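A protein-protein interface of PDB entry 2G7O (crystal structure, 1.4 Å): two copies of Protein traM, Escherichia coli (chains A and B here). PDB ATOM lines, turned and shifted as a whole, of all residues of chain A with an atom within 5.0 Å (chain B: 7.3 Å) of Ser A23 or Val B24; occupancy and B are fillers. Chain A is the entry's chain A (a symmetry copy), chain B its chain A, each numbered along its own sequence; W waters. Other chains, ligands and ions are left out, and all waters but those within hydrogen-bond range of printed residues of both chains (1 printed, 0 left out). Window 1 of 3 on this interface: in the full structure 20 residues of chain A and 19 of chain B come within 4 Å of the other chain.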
ATOM      1  N   VAL A  18       9.983 -20.713  22.674  1.00  0.00           N
ATOM      2  CA  VAL A  18       9.072 -20.259  21.624  1.00  0.00           C
ATOM      3  C   VAL A  18       8.744 -18.776  21.824  1.00  0.00           C
ATOM      4  O   VAL A  18       8.744 -17.988  20.859  1.00  0.00           O
ATOM      5  CB  VAL A  18       7.792 -21.114  21.564  1.00  0.00           C
ATOM      6  CG1 VAL A  18       6.778 -20.522  20.579  1.00  0.00           C
ATOM      7  CG2 VAL A  18       8.121 -22.564  21.203  1.00  0.00           C
ATOM      8  N   LYS A  19       8.468 -18.376  23.065  1.00  0.00           N
ATOM      9  CA  LYS A  19       8.150 -16.976  23.342  1.00  0.00           C
ATOM     10  C   LYS A  19       9.352 -16.100  23.020  1.00  0.00           C
ATOM     11  O   LYS A  19       9.204 -15.012  22.434  1.00  0.00           O
ATOM     12  CB  LYS A  19       7.705 -16.801  24.798  1.00  0.00           C
ATOM     13  CG  LYS A  19       6.985 -15.489  25.038  1.00  0.00           C
ATOM     14  CD  LYS A  19       6.334 -15.502  26.425  1.00  0.00           C
ATOM     15  CE  LYS A  19       5.561 -14.231  26.699  1.00  0.00           C
ATOM     16  NZ  LYS A  19       4.881 -14.300  28.007  1.00  0.00           N
ATOM     17  N   THR A  20      10.545 -16.533  23.421  1.00  0.00           N
ATOM     18  CA  THR A  20      11.753 -15.775  23.137  1.00  0.00           C
ATOM     19  C   THR A  20      11.979 -15.644  21.653  1.00  0.00           C
ATOM     20  O   THR A  20      12.252 -14.536  21.176  1.00  0.00           O
ATOM     21  CB  THR A  20      12.964 -16.396  23.860  1.00  0.00           C
ATOM     22  OG1 THR A  20      12.856 -16.132  25.250  1.00  0.00           O
ATOM     23  CG2 THR A  20      14.265 -15.848  23.358  1.00  0.00           C
ATOM     24  N   GLN A  21      11.859 -16.717  20.900  1.00  0.00           N
ATOM     25  CA  GLN A  21      12.120 -16.623  19.469  1.00  0.00           C
ATOM     26  C   GLN A  21      11.104 -15.681  18.795  1.00  0.00           C
ATOM     27  O   GLN A  21      11.484 -14.862  17.934  1.00  0.00           O
ATOM     28  CB  GLN A  21      12.101 -18.005  18.820  1.00  0.00           C
ATOM     29  CG  GLN A  21      12.211 -18.000  17.300  1.00  0.00           C
ATOM     30  CD  GLN A  21      13.273 -17.086  16.747  1.00  0.00           C
ATOM     31  OE1 GLN A  21      14.386 -16.966  17.288  1.00  0.00           O
ATOM     32  NE2 GLN A  21      12.935 -16.434  15.624  1.00  0.00           N
ATOM     33  N   SER A  22       9.833 -15.783  19.156  1.00  0.00           N
ATOM     34  CA  SER A  22       8.808 -14.926  18.552  1.00  0.00           C
ATOM     35  C   SER A  22       9.092 -13.451  18.872  1.00  0.00           C
ATOM     36  O   SER A  22       8.881 -12.568  18.029  1.00  0.00           O
ATOM     37  CB  SER A  22       7.422 -15.314  19.062  1.00  0.00           C
ATOM     38  OG  SER A  22       6.409 -14.587  18.391  1.00  0.00           O
ATOM     39  N   SER A  23       9.583 -13.185  20.079  1.00  0.00           N
ATOM     40  CA  SER A  23       9.874 -11.826  20.527  1.00  0.00           C
ATOM     41  C   SER A  23      11.113 -11.311  19.838  1.00  0.00           C
ATOM     42  O   SER A  23      11.136 -10.149  19.383  1.00  0.00           O
ATOM     43  CB  SER A  23      10.038 -11.793  22.045  1.00  0.00           C
ATOM     44  OG  SER A  23       8.864 -12.260  22.701  1.00  0.00           O
ATOM     45  N   VAL A  24      12.166 -12.129  19.770  1.00  0.00           N
ATOM     46  CA  VAL A  24      13.412 -11.761  19.124  1.00  0.00           C
ATOM     47  C   VAL A  24      13.201 -11.497  17.639  1.00  0.00           C
ATOM     48  O   VAL A  24      13.835 -10.595  17.085  1.00  0.00           O
ATOM     49  CB  VAL A  24      14.498 -12.849  19.407  1.00  0.00           C
ATOM     50  CG1 VAL A  24      15.660 -12.785  18.427  1.00  0.00           C
ATOM     51  CG2 VAL A  24      14.987 -12.732  20.841  1.00  0.00           C
ATOM     52  N   ALA A  25      12.334 -12.250  16.974  1.00  0.00           N
ATOM     53  CA  ALA A  25      12.046 -11.978  15.575  1.00  0.00           C
ATOM     54  C   ALA A  25      11.510 -10.558  15.387  1.00  0.00           C
ATOM     55  O   ALA A  25      11.841  -9.882  14.395  1.00  0.00           O
ATOM     56  CB  ALA A  25      11.042 -13.003  15.034  1.00  0.00           C
ATOM     57  N   LYS A  26      10.704 -10.094  16.331  1.00  0.00           N
ATOM     58  CA  LYS A  26      10.183  -8.717  16.250  1.00  0.00           C
ATOM     59  C   LYS A  26      11.246  -7.685  16.587  1.00  0.00           C
ATOM     60  O   LYS A  26      11.358  -6.651  15.913  1.00  0.00           O
ATOM     61  CB  LYS A  26       8.970  -8.544  17.159  1.00  0.00           C
ATOM     62  CG  LYS A  26       7.833  -9.459  16.703  1.00  0.00           C
ATOM     63  CD  LYS A  26       6.697  -9.533  17.675  1.00  0.00           C
ATOM     64  CE  LYS A  26       5.564 -10.416  17.112  1.00  0.00           C
ATOM     65  NZ  LYS A  26       5.954 -11.855  17.006  1.00  0.00           N
ATOM     66  N   ILE A  27      12.020  -7.937  17.632  1.00  0.00           N
ATOM     67  CA  ILE A  27      13.125  -7.047  17.976  1.00  0.00           C
ATOM     68  C   ILE A  27      14.095  -6.915  16.791  1.00  0.00           C
ATOM     69  O   ILE A  27      14.572  -5.807  16.512  1.00  0.00           O
ATOM     70  CB  ILE A  27      13.863  -7.517  19.240  1.00  0.00           C
ATOM     71  CG1 ILE A  27      12.910  -7.442  20.437  1.00  0.00           C
ATOM     72  CG2 ILE A  27      15.142  -6.699  19.493  1.00  0.00           C
ATOM     73  CD1 ILE A  27      13.315  -8.353  21.606  1.00  0.00           C
ATOM     74  N   VAL B  18      14.902 -19.064  31.207  1.00  0.00           N
ATOM     75  CA  VAL B  18      13.995 -18.217  31.981  1.00  0.00           C
ATOM     76  C   VAL B  18      14.553 -16.792  32.063  1.00  0.00           C
ATOM     77  O   VAL B  18      13.812 -15.807  31.888  1.00  0.00           O
ATOM     78  CB  VAL B  18      13.724 -18.795  33.383  1.00  0.00           C
ATOM     79  CG1 VAL B  18      12.914 -17.815  34.238  1.00  0.00           C
ATOM     80  CG2 VAL B  18      13.018 -20.150  33.287  1.00  0.00           C
ATOM     81  N   LYS B  19      15.855 -16.664  32.323  1.00  0.00           N
ATOM     82  CA  LYS B  19      16.467 -15.339  32.413  1.00  0.00           C
ATOM     83  C   LYS B  19      16.374 -14.635  31.066  1.00  0.00           C
ATOM     84  O   LYS B  19      16.074 -13.428  31.004  1.00  0.00           O
ATOM     85  CB  LYS B  19      17.921 -15.448  32.885  1.00  0.00           C
ATOM     86  CG  LYS B  19      18.477 -14.129  33.384  1.00  0.00           C
ATOM     87  CD  LYS B  19      19.816 -14.364  34.088  1.00  0.00           C
ATOM     88  CE  LYS B  19      20.394 -13.083  34.648  1.00  0.00           C
ATOM     89  NZ  LYS B  19      21.644 -13.348  35.387  1.00  0.00           N
ATOM     90  N   THR B  20      16.657 -15.352  29.982  1.00  0.00           N
ATOM     91  CA  THR B  20      16.571 -14.770  28.653  1.00  0.00           C
ATOM     92  C   THR B  20      15.165 -14.325  28.343  1.00  0.00           C
ATOM     93  O   THR B  20      14.976 -13.200  27.866  1.00  0.00           O
ATOM     94  CB  THR B  20      17.120 -15.749  27.597  1.00  0.00           C
ATOM     95  OG1 THR B  20      18.531 -15.815  27.720  1.00  0.00           O
ATOM     96  CG2 THR B  20      16.770 -15.331  26.202  1.00  0.00           C
ATOM     97  N   GLN B  21      14.170 -15.145  28.608  1.00  0.00           N
ATOM     98  CA  GLN B  21      12.806 -14.755  28.272  1.00  0.00           C
ATOM     99  C   GLN B  21      12.384 -13.515  29.084  1.00  0.00           C
ATOM    100  O   GLN B  21      11.752 -12.591  28.534  1.00  0.00           O
ATOM    101  CB  GLN B  21      11.837 -15.913  28.495  1.00  0.00           C
ATOM    102  CG  GLN B  21      10.366 -15.559  28.318  1.00  0.00           C
ATOM    103  CD  GLN B  21      10.056 -14.737  27.095  1.00  0.00           C
ATOM    104  OE1 GLN B  21      10.612 -14.948  26.002  1.00  0.00           O
ATOM    105  NE2 GLN B  21       9.127 -13.784  27.268  1.00  0.00           N
ATOM    106  N   SER B  22      12.707 -13.479  30.369  1.00  0.00           N
ATOM    107  CA  SER B  22      12.331 -12.336  31.208  1.00  0.00           C
ATOM    108  C   SER B  22      13.005 -11.056  30.694  1.00  0.00           C
ATOM    109  O   SER B  22      12.406  -9.972  30.715  1.00  0.00           O
ATOM    110  CB  SER B  22      12.728 -12.589  32.660  1.00  0.00           C
ATOM    111  OG  SER B  22      12.256 -11.556  33.505  1.00  0.00           O
ATOM    112  N   SER B  23      14.242 -11.179  30.219  1.00  0.00           N
ATOM    113  CA  SER B  23      15.011 -10.042  29.723  1.00  0.00           C
ATOM    114  C   SER B  23      14.472  -9.599  28.385  1.00  0.00           C
ATOM    115  O   SER B  23      14.317  -8.383  28.148  1.00  0.00           O
ATOM    116  CB  SER B  23      16.491 -10.407  29.623  1.00  0.00           C
ATOM    117  OG  SER B  23      17.010 -10.808  30.887  1.00  0.00           O
ATOM    118  N   VAL B  24      14.206 -10.546  27.483  1.00  0.00           N
ATOM    119  CA  VAL B  24      13.672 -10.256  26.166  1.00  0.00           C
ATOM    120  C   VAL B  24      12.298  -9.606  26.264  1.00  0.00           C
ATOM    121  O   VAL B  24      11.984  -8.722  25.463  1.00  0.00           O
ATOM    122  CB  VAL B  24      13.679 -11.552  25.292  1.00  0.00           C
ATOM    123  CG1 VAL B  24      12.747 -11.455  24.094  1.00  0.00           C
ATOM    124  CG2 VAL B  24      15.099 -11.873  24.855  1.00  0.00           C
ATOM    125  N   ALA B  25      11.467 -10.013  27.215  1.00  0.00           N
ATOM    126  CA  ALA B  25      10.178  -9.364  27.391  1.00  0.00           C
ATOM    127  C   ALA B  25      10.345  -7.870  27.671  1.00  0.00           C
ATOM    128  O   ALA B  25       9.550  -7.042  27.188  1.00  0.00           O
ATOM    129  CB  ALA B  25       9.399 -10.037  28.528  1.00  0.00           C
ATOM    130  N   LYS B  26      11.373  -7.516  28.429  1.00  0.00           N
ATOM    131  CA  LYS B  26      11.633  -6.091  28.706  1.00  0.00           C
ATOM    132  C   LYS B  26      12.215  -5.373  27.501  1.00  0.00           C
ATOM    133  O   LYS B  26      11.817  -4.242  27.186  1.00  0.00           O
ATOM    134  CB  LYS B  26      12.555  -5.935  29.912  1.00  0.00           C
ATOM    135  CG  LYS B  26      11.886  -6.500  31.165  1.00  0.00           C
ATOM    136  CD  LYS B  26      12.808  -6.609  32.339  1.00  0.00           C
ATOM    137  CE  LYS B  26      12.043  -7.118  33.579  1.00  0.00           C
ATOM    138  NZ  LYS B  26      11.586  -8.533  33.432  1.00  0.00           N
ATOM    139  N   ILE B  27      13.167  -6.002  26.827  1.00  0.00           N
ATOM    140  CA  ILE B  27      13.721  -5.428  25.605  1.00  0.00           C
ATOM    141  C   ILE B  27      12.606  -5.184  24.575  1.00  0.00           C
ATOM    142  O   ILE B  27      12.609  -4.142  23.905  1.00  0.00           O
ATOM    143  CB  ILE B  27      14.831  -6.311  25.013  1.00  0.00           C
ATOM    144  CG1 ILE B  27      16.009  -6.364  25.992  1.00  0.00           C
ATOM    145  CG2 ILE B  27      15.279  -5.815  23.627  1.00  0.00           C
ATOM    146  CD1 ILE B  27      16.917  -7.588  25.798  1.00  0.00           C
ATOM    147  N   LEU B  28      11.643  -6.085  24.443  1.00  0.00           N
ATOM    148  CA  LEU B  28      10.533  -5.921  23.512  1.00  0.00           C
ATOM    149  C   LEU B  28       9.740  -4.677  23.880  1.00  0.00           C
ATOM    150  O   LEU B  28       9.365  -3.889  23.008  1.00  0.00           O
ATOM    151  CB  LEU B  28       9.636  -7.167  23.527  1.00  0.00           C
ATOM    152  CG  LEU B  28       8.482  -7.135  22.518  1.00  0.00           C
ATOM    153  CD1 LEU B  28       8.968  -7.244  21.077  1.00  0.00           C
ATOM    154  CD2 LEU B  28       7.466  -8.254  22.803  1.00  0.00           C
ATOM    155  N   GLY B  29       9.466  -4.488  25.165  1.00  0.00           N
ATOM    156  CA  GLY B  29       8.726  -3.301  25.590  1.00  0.00           C
ATOM    157  C   GLY B  29       9.503  -2.034  25.285  1.00  0.00           C
ATOM    158  O   GLY B  29       8.924  -1.046  24.799  1.00  0.00           O
ATOM    159  N   ILE B  30      10.803  -2.020  25.588  1.00  0.00           N
ATOM    160  CA  ILE B  30      11.606  -0.819  25.298  1.00  0.00           C
ATOM    161  C   ILE B  30      11.624  -0.526  23.793  1.00  0.00           C
ATOM    162  O   ILE B  30      11.462   0.630  23.374  1.00  0.00           O
ATOM    163  CB  ILE B  30      13.033  -0.975  25.847  1.00  0.00           C
ATOM    164  CG1 ILE B  30      12.999  -1.022  27.389  1.00  0.00           C
ATOM    165  CG2 ILE B  30      13.931   0.177  25.343  1.00  0.00           C
ATOM    166  CD1 ILE B  30      14.332  -1.478  28.035  1.00  0.00           C
ATOM    167  N   MET B  48       2.001  -6.825  18.907  1.00  0.00           N
ATOM    168  CA  MET B  48       3.093  -7.790  19.073  1.00  0.00           C
ATOM    169  C   MET B  48       2.778  -8.864  20.118  1.00  0.00           C
ATOM    170  O   MET B  48       3.018 -10.063  19.886  1.00  0.00           O
ATOM    171  CB  MET B  48       4.407  -7.083  19.404  1.00  0.00           C
ATOM    172  CG  MET B  48       4.897  -6.204  18.248  1.00  0.00           C
ATOM    173  SD  MET B  48       6.616  -5.701  18.450  1.00  0.00           S
ATOM    174  CE  MET B  48       6.528  -4.696  19.923  1.00  0.00           C
ATOM    175  N   ILE B  52       2.587 -12.906  19.511  1.00  0.00           N
ATOM    176  CA  ILE B  52       3.430 -13.813  20.300  1.00  0.00           C
ATOM    177  C   ILE B  52       2.568 -14.811  21.071  1.00  0.00           C
ATOM    178  O   ILE B  52       2.864 -16.012  21.081  1.00  0.00           O
ATOM    179  CB  ILE B  52       4.341 -13.005  21.253  1.00  0.00           C
ATOM    180  CG1 ILE B  52       5.366 -12.189  20.441  1.00  0.00           C
ATOM    181  CG2 ILE B  52       5.045 -13.924  22.271  1.00  0.00           C
ATOM    182  CD1 ILE B  52       5.962 -11.037  21.213  1.00  0.00           C
ATOM    183  N   VAL B  56       2.874 -18.945  20.782  1.00  0.00           N
ATOM    184  CA  VAL B  56       3.197 -19.777  21.938  1.00  0.00           C
ATOM    185  C   VAL B  56       2.043 -20.763  22.198  1.00  0.00           C
ATOM    186  O   VAL B  56       2.268 -21.955  22.405  1.00  0.00           O
ATOM    187  CB  VAL B  56       3.469 -18.929  23.195  1.00  0.00           C
ATOM    188  CG1 VAL B  56       3.639 -19.830  24.409  1.00  0.00           C
ATOM    189  CG2 VAL B  56       4.694 -18.025  22.976  1.00  0.00           C
HETATM  190  O   HOH W   1       8.530 -11.580  25.354  1.00  0.00           O
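OE1 of Gln B21 is in hydrogen-bond range of OG1 of Thr A20.
Lys A19 touches Gln B21, but with the chains exchanged Gln A21 does not touch Lys B19 (11.3 Å). Thr B20 touches its own counterpart, Thr A20. Ser A23 touches Val B24, but with the chains exchanged Val A24 does not touch Ser B23 (8.2 Å). Ile A27 touches its own counterpart, Ile B27. 10 positions are printed for both chains.
Of the 10 printed residues of chain A, 7 touch a printed residue of chain B. Hydrophobic or aromatic side chains of chain A within 4 Å of the printed part of chain B: Val A18 and Ile A27. Of the 16 printed residues of chain B, 8 touch a printed residue of chain A. Among the printed residues, 13 pairs touch across the chains.
Among the printed residues, pairs that only touch across the chains: Val A18 with Val B56 (3.9 Å), Lys A19 with Gln B21 (3.4 Å), Lys A19 with Ile B52 (3.7 Å), Lys A19 with Val B56 (3.6 Å), Thr A20 with Thr B20 (3.8 Å), Ser A22 with Ile B52 (3.3 Å), Ser A23 with Val B24 (3.4 Å), Ser A23 with Ile B52 (3.5 Å), Lys A26 with Met B48 (3.8 Å), Lys A26 with Ile B52 (3.5 Å), Ile A27 with Ile B27 (3.8 Å) and Ile A27 with Leu B28 (3.998 Å).
Water W1 bridges OG of Ser A23 and NE2 of Gln B21.
The side-chain hydroxyl (OG) of Ser A23 lies within hydrogen-bond range of the backbone carbonyl oxygen (O) of Lys A19 (2.8 Å). The side-chain hydroxyl (OG) of Ser A22 lies within hydrogen-bond range of the side-chain amino group (NZ) of Lys A26.
Printed residues of chain B within 4 Å of Val A18: Val B56. Printed residues of chain B within 4 Å of Ser A22: Ile B52 (3.3 Å). Of the printed residues of chain B, Ser A23 touches Val B24 (3.4 Å) and Ile B52 (3.5 Å). Printed residues of chain A within 4 Å of Val B24: Ser A23. Of the printed residues of chain A, Leu B28 touches Ile A27. Of the printed residues of chain A, Met B48 touches Lys A26 (3.8 Å). The nearest printed residue of chain A that does not touch Val B24 is Ile A27 (4.02 Å).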
